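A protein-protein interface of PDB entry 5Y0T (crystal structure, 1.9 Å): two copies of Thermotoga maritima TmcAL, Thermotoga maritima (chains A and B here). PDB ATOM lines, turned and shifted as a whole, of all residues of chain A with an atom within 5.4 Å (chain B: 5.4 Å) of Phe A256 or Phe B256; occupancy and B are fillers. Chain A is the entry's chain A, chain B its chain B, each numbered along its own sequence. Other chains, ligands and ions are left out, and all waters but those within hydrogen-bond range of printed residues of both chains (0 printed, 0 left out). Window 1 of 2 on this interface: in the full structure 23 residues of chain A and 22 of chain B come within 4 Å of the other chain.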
ATOM      1  N   MET A 253     -17.255  19.284 -17.833  1.00  0.00           N
ATOM      2  CA  MET A 253     -15.823  19.537 -18.005  1.00  0.00           C
ATOM      3  C   MET A 253     -15.194  20.252 -16.811  1.00  0.00           C
ATOM      4  O   MET A 253     -13.995  20.527 -16.805  1.00  0.00           O
ATOM      5  CB  MET A 253     -15.575  20.377 -19.248  1.00  0.00           C
ATOM      6  CG  MET A 253     -15.970  19.690 -20.526  1.00  0.00           C
ATOM      7  SD  MET A 253     -15.962  20.808 -21.931  1.00  0.00           S
ATOM      8  CE  MET A 253     -16.332  19.598 -23.203  1.00  0.00           C
ATOM      9  N   GLY A 254     -16.013  20.586 -15.825  1.00  0.00           N
ATOM     10  CA  GLY A 254     -15.575  21.465 -14.758  1.00  0.00           C
ATOM     11  C   GLY A 254     -14.424  20.903 -13.934  1.00  0.00           C
ATOM     12  O   GLY A 254     -13.446  21.608 -13.660  1.00  0.00           O
ATOM     13  N   ASP A 255     -14.528  19.643 -13.522  1.00  0.00           N
ATOM     14  CA  ASP A 255     -13.467  19.077 -12.691  1.00  0.00           C
ATOM     15  C   ASP A 255     -12.163  19.001 -13.487  1.00  0.00           C
ATOM     16  O   ASP A 255     -11.090  19.215 -12.914  1.00  0.00           O
ATOM     17  CB  ASP A 255     -13.834  17.688 -12.147  1.00  0.00           C
ATOM     18  CG  ASP A 255     -14.677  17.743 -10.875  1.00  0.00           C
ATOM     19  OD1 ASP A 255     -14.977  18.848 -10.370  1.00  0.00           O
ATOM     20  OD2 ASP A 255     -15.025  16.664 -10.355  1.00  0.00           O
ATOM     21  N   PHE A 256     -12.241  18.720 -14.796  1.00  0.00           N
ATOM     22  CA  PHE A 256     -11.020  18.718 -15.601  1.00  0.00           C
ATOM     23  C   PHE A 256     -10.363  20.091 -15.599  1.00  0.00           C
ATOM     24  O   PHE A 256      -9.164  20.203 -15.345  1.00  0.00           O
ATOM     25  CB  PHE A 256     -11.240  18.299 -17.068  1.00  0.00           C
ATOM     26  CG  PHE A 256      -9.941  18.127 -17.809  1.00  0.00           C
ATOM     27  CD1 PHE A 256      -9.309  19.210 -18.394  1.00  0.00           C
ATOM     28  CD2 PHE A 256      -9.311  16.894 -17.846  1.00  0.00           C
ATOM     29  CE1 PHE A 256      -8.084  19.062 -19.024  1.00  0.00           C
ATOM     30  CE2 PHE A 256      -8.080  16.737 -18.482  1.00  0.00           C
ATOM     31  CZ  PHE A 256      -7.472  17.818 -19.062  1.00  0.00           C
ATOM     32  N   LEU A 257     -11.144  21.121 -15.913  1.00  0.00           N
ATOM     33  CA  LEU A 257     -10.617  22.478 -16.012  1.00  0.00           C
ATOM     34  C   LEU A 257      -9.968  22.903 -14.701  1.00  0.00           C
ATOM     35  O   LEU A 257      -8.835  23.404 -14.670  1.00  0.00           O
ATOM     36  CB  LEU A 257     -11.740  23.454 -16.391  1.00  0.00           C
ATOM     37  CG  LEU A 257     -12.272  23.256 -17.805  1.00  0.00           C
ATOM     38  CD1 LEU A 257     -13.466  24.168 -18.070  1.00  0.00           C
ATOM     39  CD2 LEU A 257     -11.170  23.491 -18.811  1.00  0.00           C
ATOM     40  N   LEU A 258     -10.682  22.663 -13.607  1.00  0.00           N
ATOM     41  CA  LEU A 258     -10.208  23.095 -12.308  1.00  0.00           C
ATOM     42  C   LEU A 258      -8.929  22.341 -11.934  1.00  0.00           C
ATOM     43  O   LEU A 258      -7.961  22.945 -11.451  1.00  0.00           O
ATOM     44  CB  LEU A 258     -11.297  22.905 -11.243  1.00  0.00           C
ATOM     45  CG  LEU A 258     -10.883  23.267  -9.806  1.00  0.00           C
ATOM     46  CD1 LEU A 258     -10.360  24.698  -9.749  1.00  0.00           C
ATOM     47  CD2 LEU A 258     -12.049  23.089  -8.829  1.00  0.00           C
ATOM     48  N   SER A 259      -8.923  21.033 -12.175  1.00  0.00           N
ATOM     49  CA  SER A 259      -7.759  20.208 -11.864  1.00  0.00           C
ATOM     50  C   SER A 259      -6.562  20.609 -12.730  1.00  0.00           C
ATOM     51  O   SER A 259      -5.427  20.676 -12.265  1.00  0.00           O
ATOM     52  CB  SER A 259      -8.083  18.719 -12.063  1.00  0.00           C
ATOM     53  OG  SER A 259      -9.045  18.270 -11.123  1.00  0.00           O
ATOM     54  N   PHE A 260      -6.830  20.882 -13.995  1.00  0.00           N
ATOM     55  CA  PHE A 260      -5.794  21.306 -14.928  1.00  0.00           C
ATOM     56  C   PHE A 260      -5.146  22.632 -14.452  1.00  0.00           C
ATOM     57  O   PHE A 260      -3.923  22.771 -14.463  1.00  0.00           O
ATOM     58  CB  PHE A 260      -6.410  21.424 -16.336  1.00  0.00           C
ATOM     59  CG  PHE A 260      -5.443  21.864 -17.404  1.00  0.00           C
ATOM     60  CD1 PHE A 260      -5.217  23.216 -17.635  1.00  0.00           C
ATOM     61  CD2 PHE A 260      -4.787  20.934 -18.197  1.00  0.00           C
ATOM     62  CE1 PHE A 260      -4.329  23.632 -18.615  1.00  0.00           C
ATOM     63  CE2 PHE A 260      -3.892  21.348 -19.190  1.00  0.00           C
ATOM     64  CZ  PHE A 260      -3.667  22.703 -19.392  1.00  0.00           C
ATOM     65  N   PHE A 261      -5.948  23.577 -13.966  1.00  0.00           N
ATOM     66  CA  PHE A 261      -5.391  24.860 -13.507  1.00  0.00           C
ATOM     67  C   PHE A 261      -4.506  24.698 -12.272  1.00  0.00           C
ATOM     68  O   PHE A 261      -3.612  25.503 -12.052  1.00  0.00           O
ATOM     69  CB  PHE A 261      -6.499  25.885 -13.220  1.00  0.00           C
ATOM     70  CG  PHE A 261      -7.387  26.148 -14.401  1.00  0.00           C
ATOM     71  CD1 PHE A 261      -6.912  25.957 -15.688  1.00  0.00           C
ATOM     72  CD2 PHE A 261      -8.703  26.538 -14.226  1.00  0.00           C
ATOM     73  CE1 PHE A 261      -7.726  26.165 -16.792  1.00  0.00           C
ATOM     74  CE2 PHE A 261      -9.525  26.741 -15.322  1.00  0.00           C
ATOM     75  CZ  PHE A 261      -9.041  26.557 -16.607  1.00  0.00           C
ATOM     76  N   LEU A 263      -2.355  22.527 -12.001  1.00  0.00           N
ATOM     77  CA  LEU A 263      -1.097  22.015 -12.514  1.00  0.00           C
ATOM     78  C   LEU A 263      -0.213  23.154 -13.022  1.00  0.00           C
ATOM     79  O   LEU A 263       0.966  22.950 -13.320  1.00  0.00           O
ATOM     80  CB  LEU A 263      -1.364  20.999 -13.641  1.00  0.00           C
ATOM     81  CG  LEU A 263      -2.161  19.744 -13.233  1.00  0.00           C
ATOM     82  CD1 LEU A 263      -2.465  18.832 -14.448  1.00  0.00           C
ATOM     83  CD2 LEU A 263      -1.412  18.978 -12.139  1.00  0.00           C
ATOM     84  N   VAL A 318      -6.775  25.694 -21.241  1.00  0.00           N
ATOM     85  CA  VAL A 318      -6.698  24.243 -21.363  1.00  0.00           C
ATOM     86  C   VAL A 318      -6.190  23.831 -22.752  1.00  0.00           C
ATOM     87  O   VAL A 318      -5.531  22.802 -22.896  1.00  0.00           O
ATOM     88  CB  VAL A 318      -8.062  23.590 -21.057  1.00  0.00           C
ATOM     89  CG1 VAL A 318      -9.008  23.695 -22.256  1.00  0.00           C
ATOM     90  CG2 VAL A 318      -7.876  22.148 -20.657  1.00  0.00           C
ATOM     91  N   PHE A 397     -10.775  16.399 -27.315  1.00  0.00           N
ATOM     92  CA  PHE A 397     -11.020  16.689 -25.915  1.00  0.00           C
ATOM     93  C   PHE A 397     -12.519  16.631 -25.620  1.00  0.00           C
ATOM     94  O   PHE A 397     -12.963  15.972 -24.686  1.00  0.00           O
ATOM     95  CB  PHE A 397     -10.450  18.058 -25.566  1.00  0.00           C
ATOM     96  CG  PHE A 397     -10.699  18.487 -24.142  1.00  0.00           C
ATOM     97  CD1 PHE A 397      -9.911  17.998 -23.110  1.00  0.00           C
ATOM     98  CD2 PHE A 397     -11.705  19.408 -23.841  1.00  0.00           C
ATOM     99  CE1 PHE A 397     -10.133  18.411 -21.782  1.00  0.00           C
ATOM    100  CE2 PHE A 397     -11.936  19.826 -22.525  1.00  0.00           C
ATOM    101  CZ  PHE A 397     -11.146  19.335 -21.496  1.00  0.00           C
ATOM    102  N   PHE A 401     -16.053  13.763 -23.179  1.00  0.00           N
ATOM    103  CA  PHE A 401     -17.198  14.122 -22.333  1.00  0.00           C
ATOM    104  C   PHE A 401     -18.564  13.681 -22.862  1.00  0.00           C
ATOM    105  O   PHE A 401     -19.590  13.990 -22.251  1.00  0.00           O
ATOM    106  CB  PHE A 401     -17.164  15.626 -22.060  1.00  0.00           C
ATOM    107  CG  PHE A 401     -15.906  16.043 -21.366  1.00  0.00           C
ATOM    108  CD1 PHE A 401     -15.824  16.008 -19.981  1.00  0.00           C
ATOM    109  CD2 PHE A 401     -14.779  16.378 -22.101  1.00  0.00           C
ATOM    110  CE1 PHE A 401     -14.645  16.345 -19.328  1.00  0.00           C
ATOM    111  CE2 PHE A 401     -13.594  16.720 -21.470  1.00  0.00           C
ATOM    112  CZ  PHE A 401     -13.529  16.711 -20.068  1.00  0.00           C
ATOM    113  N   MET B 253      -8.766   8.911 -11.422  1.00  0.00           N
ATOM    114  CA  MET B 253      -7.997   9.910 -12.157  1.00  0.00           C
ATOM    115  C   MET B 253      -7.882   9.587 -13.649  1.00  0.00           C
ATOM    116  O   MET B 253      -7.272  10.342 -14.414  1.00  0.00           O
ATOM    117  CB  MET B 253      -6.584  10.026 -11.567  1.00  0.00           C
ATOM    118  CG  MET B 253      -6.549  10.467 -10.121  1.00  0.00           C
ATOM    119  SD  MET B 253      -4.877  10.329  -9.458  1.00  0.00           S
ATOM    120  CE  MET B 253      -5.192  11.101  -7.867  1.00  0.00           C
ATOM    121  N   GLY B 254      -8.449   8.457 -14.054  1.00  0.00           N
ATOM    122  CA  GLY B 254      -8.247   7.952 -15.396  1.00  0.00           C
ATOM    123  C   GLY B 254      -8.727   8.841 -16.531  1.00  0.00           C
ATOM    124  O   GLY B 254      -8.014   9.043 -17.522  1.00  0.00           O
ATOM    125  N   ASP B 255      -9.944   9.348 -16.411  1.00  0.00           N
ATOM    126  CA  ASP B 255     -10.486  10.231 -17.439  1.00  0.00           C
ATOM    127  C   ASP B 255      -9.665  11.515 -17.528  1.00  0.00           C
ATOM    128  O   ASP B 255      -9.463  12.035 -18.624  1.00  0.00           O
ATOM    129  CB  ASP B 255     -11.948  10.566 -17.159  1.00  0.00           C
ATOM    130  CG  ASP B 255     -12.904   9.532 -17.711  1.00  0.00           C
ATOM    131  OD1 ASP B 255     -12.447   8.470 -18.196  1.00  0.00           O
ATOM    132  OD2 ASP B 255     -14.126   9.788 -17.652  1.00  0.00           O
ATOM    133  N   PHE B 256      -9.188  12.031 -16.392  1.00  0.00           N
ATOM    134  CA  PHE B 256      -8.320  13.214 -16.458  1.00  0.00           C
ATOM    135  C   PHE B 256      -7.059  12.939 -17.279  1.00  0.00           C
ATOM    136  O   PHE B 256      -6.680  13.724 -18.155  1.00  0.00           O
ATOM    137  CB  PHE B 256      -7.868  13.720 -15.070  1.00  0.00           C
ATOM    138  CG  PHE B 256      -7.097  15.004 -15.168  1.00  0.00           C
ATOM    139  CD1 PHE B 256      -7.756  16.226 -15.089  1.00  0.00           C
ATOM    140  CD2 PHE B 256      -5.738  14.999 -15.462  1.00  0.00           C
ATOM    141  CE1 PHE B 256      -7.063  17.423 -15.248  1.00  0.00           C
ATOM    142  CE2 PHE B 256      -5.043  16.176 -15.636  1.00  0.00           C
ATOM    143  CZ  PHE B 256      -5.710  17.402 -15.521  1.00  0.00           C
ATOM    144  N   LEU B 257      -6.378  11.851 -16.936  1.00  0.00           N
ATOM    145  CA  LEU B 257      -5.121  11.486 -17.590  1.00  0.00           C
ATOM    146  C   LEU B 257      -5.320  11.301 -19.090  1.00  0.00           C
ATOM    147  O   LEU B 257      -4.554  11.815 -19.907  1.00  0.00           O
ATOM    148  CB  LEU B 257      -4.556  10.201 -16.963  1.00  0.00           C
ATOM    149  CG  LEU B 257      -4.139  10.343 -15.492  1.00  0.00           C
ATOM    150  CD1 LEU B 257      -3.754   8.984 -14.879  1.00  0.00           C
ATOM    151  CD2 LEU B 257      -2.985  11.291 -15.372  1.00  0.00           C
ATOM    152  N   LEU B 258      -6.363  10.569 -19.454  1.00  0.00           N
ATOM    153  CA  LEU B 258      -6.577  10.247 -20.852  1.00  0.00           C
ATOM    154  C   LEU B 258      -6.945  11.523 -21.624  1.00  0.00           C
ATOM    155  O   LEU B 258      -6.428  11.766 -22.718  1.00  0.00           O
ATOM    156  CB  LEU B 258      -7.661   9.182 -20.995  1.00  0.00           C
ATOM    157  CG  LEU B 258      -8.058   8.809 -22.422  1.00  0.00           C
ATOM    158  CD1 LEU B 258      -6.829   8.430 -23.222  1.00  0.00           C
ATOM    159  CD2 LEU B 258      -9.073   7.663 -22.413  1.00  0.00           C
ATOM    160  N   SER B 259      -7.816  12.347 -21.047  1.00  0.00           N
ATOM    161  CA  SER B 259      -8.195  13.612 -21.693  1.00  0.00           C
ATOM    162  C   SER B 259      -6.973  14.527 -21.854  1.00  0.00           C
ATOM    163  O   SER B 259      -6.783  15.175 -22.893  1.00  0.00           O
ATOM    164  CB  SER B 259      -9.286  14.332 -20.890  1.00  0.00           C
ATOM    165  OG  SER B 259     -10.464  13.540 -20.801  1.00  0.00           O
ATOM    166  N   PHE B 260      -6.153  14.574 -20.809  1.00  0.00           N
ATOM    167  CA  PHE B 260      -4.932  15.383 -20.804  1.00  0.00           C
ATOM    168  C   PHE B 260      -4.008  14.964 -21.955  1.00  0.00           C
ATOM    169  O   PHE B 260      -3.447  15.805 -22.650  1.00  0.00           O
ATOM    170  CB  PHE B 260      -4.220  15.241 -19.447  1.00  0.00           C
ATOM    171  CG  PHE B 260      -2.993  16.120 -19.282  1.00  0.00           C
ATOM    172  CD1 PHE B 260      -1.734  15.649 -19.643  1.00  0.00           C
ATOM    173  CD2 PHE B 260      -3.098  17.393 -18.725  1.00  0.00           C
ATOM    174  CE1 PHE B 260      -0.603  16.437 -19.480  1.00  0.00           C
ATOM    175  CE2 PHE B 260      -1.964  18.198 -18.549  1.00  0.00           C
ATOM    176  CZ  PHE B 260      -0.718  17.719 -18.932  1.00  0.00           C
ATOM    177  N   PHE B 261      -3.843  13.660 -22.155  1.00  0.00           N
ATOM    178  CA  PHE B 261      -2.986  13.190 -23.250  1.00  0.00           C
ATOM    179  C   PHE B 261      -3.527  13.615 -24.624  1.00  0.00           C
ATOM    180  O   PHE B 261      -2.759  13.805 -25.562  1.00  0.00           O
ATOM    181  CB  PHE B 261      -2.809  11.670 -23.185  1.00  0.00           C
ATOM    182  CG  PHE B 261      -2.184  11.190 -21.904  1.00  0.00           C
ATOM    183  CD1 PHE B 261      -1.351  12.029 -21.166  1.00  0.00           C
ATOM    184  CD2 PHE B 261      -2.436   9.913 -21.427  1.00  0.00           C
ATOM    185  CE1 PHE B 261      -0.770  11.606 -19.972  1.00  0.00           C
ATOM    186  CE2 PHE B 261      -1.871   9.484 -20.230  1.00  0.00           C
ATOM    187  CZ  PHE B 261      -1.032  10.334 -19.504  1.00  0.00           C
ATOM    188  N   LEU B 263      -4.540  16.447 -25.262  1.00  0.00           N
ATOM    189  CA  LEU B 263      -4.186  17.860 -25.428  1.00  0.00           C
ATOM    190  C   LEU B 263      -2.742  18.027 -25.919  1.00  0.00           C
ATOM    191  O   LEU B 263      -2.312  19.127 -26.267  1.00  0.00           O
ATOM    192  CB  LEU B 263      -4.374  18.604 -24.107  1.00  0.00           C
ATOM    193  CG  LEU B 263      -5.789  18.572 -23.531  1.00  0.00           C
ATOM    194  CD1 LEU B 263      -5.791  19.146 -22.095  1.00  0.00           C
ATOM    195  CD2 LEU B 263      -6.729  19.372 -24.439  1.00  0.00           C
ATOM    196  N   VAL B 318       1.497  14.314 -16.660  1.00  0.00           N
ATOM    197  CA  VAL B 318       0.578  15.351 -16.167  1.00  0.00           C
ATOM    198  C   VAL B 318       1.276  16.359 -15.277  1.00  0.00           C
ATOM    199  O   VAL B 318       0.877  17.519 -15.240  1.00  0.00           O
ATOM    200  CB  VAL B 318      -0.623  14.809 -15.371  1.00  0.00           C
ATOM    201  CG1 VAL B 318      -1.666  14.276 -16.304  1.00  0.00           C
ATOM    202  CG2 VAL B 318      -0.180  13.798 -14.297  1.00  0.00           C
ATOM    203  N   PHE B 397      -3.249  18.386  -6.858  1.00  0.00           N
ATOM    204  CA  PHE B 397      -3.929  17.615  -7.902  1.00  0.00           C
ATOM    205  C   PHE B 397      -4.707  16.477  -7.272  1.00  0.00           C
ATOM    206  O   PHE B 397      -5.871  16.259  -7.577  1.00  0.00           O
ATOM    207  CB  PHE B 397      -2.921  17.076  -8.911  1.00  0.00           C
ATOM    208  CG  PHE B 397      -3.531  16.257 -10.005  1.00  0.00           C
ATOM    209  CD1 PHE B 397      -4.251  16.870 -11.032  1.00  0.00           C
ATOM    210  CD2 PHE B 397      -3.347  14.873 -10.048  1.00  0.00           C
ATOM    211  CE1 PHE B 397      -4.788  16.111 -12.076  1.00  0.00           C
ATOM    212  CE2 PHE B 397      -3.892  14.115 -11.098  1.00  0.00           C
ATOM    213  CZ  PHE B 397      -4.612  14.740 -12.097  1.00  0.00           C
ATOM    214  N   PHE B 401      -9.455  14.690  -6.199  1.00  0.00           N
ATOM    215  CA  PHE B 401     -10.064  13.366  -6.319  1.00  0.00           C
ATOM    216  C   PHE B 401     -10.588  12.797  -5.002  1.00  0.00           C
ATOM    217  O   PHE B 401     -11.009  11.646  -4.960  1.00  0.00           O
ATOM    218  CB  PHE B 401      -9.072  12.420  -7.004  1.00  0.00           C
ATOM    219  CG  PHE B 401      -8.749  12.866  -8.385  1.00  0.00           C
ATOM    220  CD1 PHE B 401      -9.548  12.472  -9.453  1.00  0.00           C
ATOM    221  CD2 PHE B 401      -7.716  13.765  -8.612  1.00  0.00           C
ATOM    222  CE1 PHE B 401      -9.287  12.917 -10.736  1.00  0.00           C
ATOM    223  CE2 PHE B 401      -7.450  14.227  -9.889  1.00  0.00           C
ATOM    224  CZ  PHE B 401      -8.231  13.801 -10.957  1.00  0.00           C
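O of Asp B255 sits at hydrogen-bond distance from OG of Ser B259, 2.8 Å away.
The backbone carbonyl oxygen (O) of Asp A255 lies within hydrogen-bond range of the side-chain hydroxyl (OG) of Ser A259 (2.9 Å).
Phe A256 touches Ser B259.
Phe A256 touches Phe B260.
CZ of Phe A256 touches CD1 of Leu B263, at 3.7 Å.
Ser A259 touches Phe B256 (CB to CE1, 3.6 Å).
Phe A260 touches Phe B256 (N to CE1, 3.7 Å).
Phe B260 touches Phe A260.
Leu A263 touches Phe B256 (CD1 to CZ, 3.7 Å).
Leu A263 touches Val B318 (CD1 to O, 3.7 Å).
Leu A263 touches Phe B397.
Phe A397 touches Leu B263.
Of chain A, only Phe A256 (3.2 Å), Ser A259 (3.6 Å), Phe A260 (3.7 Å) and Leu A263 (3.7 Å) come within 4 Å of Phe B256.
Printed residues of chain A within 4 Å of Phe B260: Phe A256 (3.7 Å) and Phe A260 (3.7 Å).
Of the printed residues of chain A, Val B318 touches Leu A263 (3.7 Å).
Of the printed residues of chain A, Leu B263 touches Phe A256 (3.7 Å), Val A318 (3.8 Å) and Phe A397 (3.7 Å).
Printed residues of chain B within 4 Å of Val A318: Leu B263.
The nearest residue of chain B that does not touch Phe A256 is Asp B255 (4.9 Å).
Of the 13 printed residues of chain B, 6 touch a printed residue of chain A.
Printed residues of chain B that touch a printed residue of chain A: Phe B256, Ser B259, Phe B260, Leu B263, Val B318 and Phe B397.
Among the printed residues, no Asp or Glu carboxylate lies within 4 Å of a Lys or Arg side-chain nitrogen of the other chain.
Phe A256 touches Ser B259, and with the chains exchanged Ser A259 touches Phe B256.
Phe A260 touches its own counterpart, Phe B260.
Leu A263 touches Val B318, and with the chains exchanged Val A318 touches Leu B263.
Leu A263 touches Phe B397, and with the chains exchanged Phe A397 touches Leu B263.
13 positions are printed for both chains.
Of the 12 pairs that touch across the chains among the printed residues, 12 have their exchanged pair printed and touching as well.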
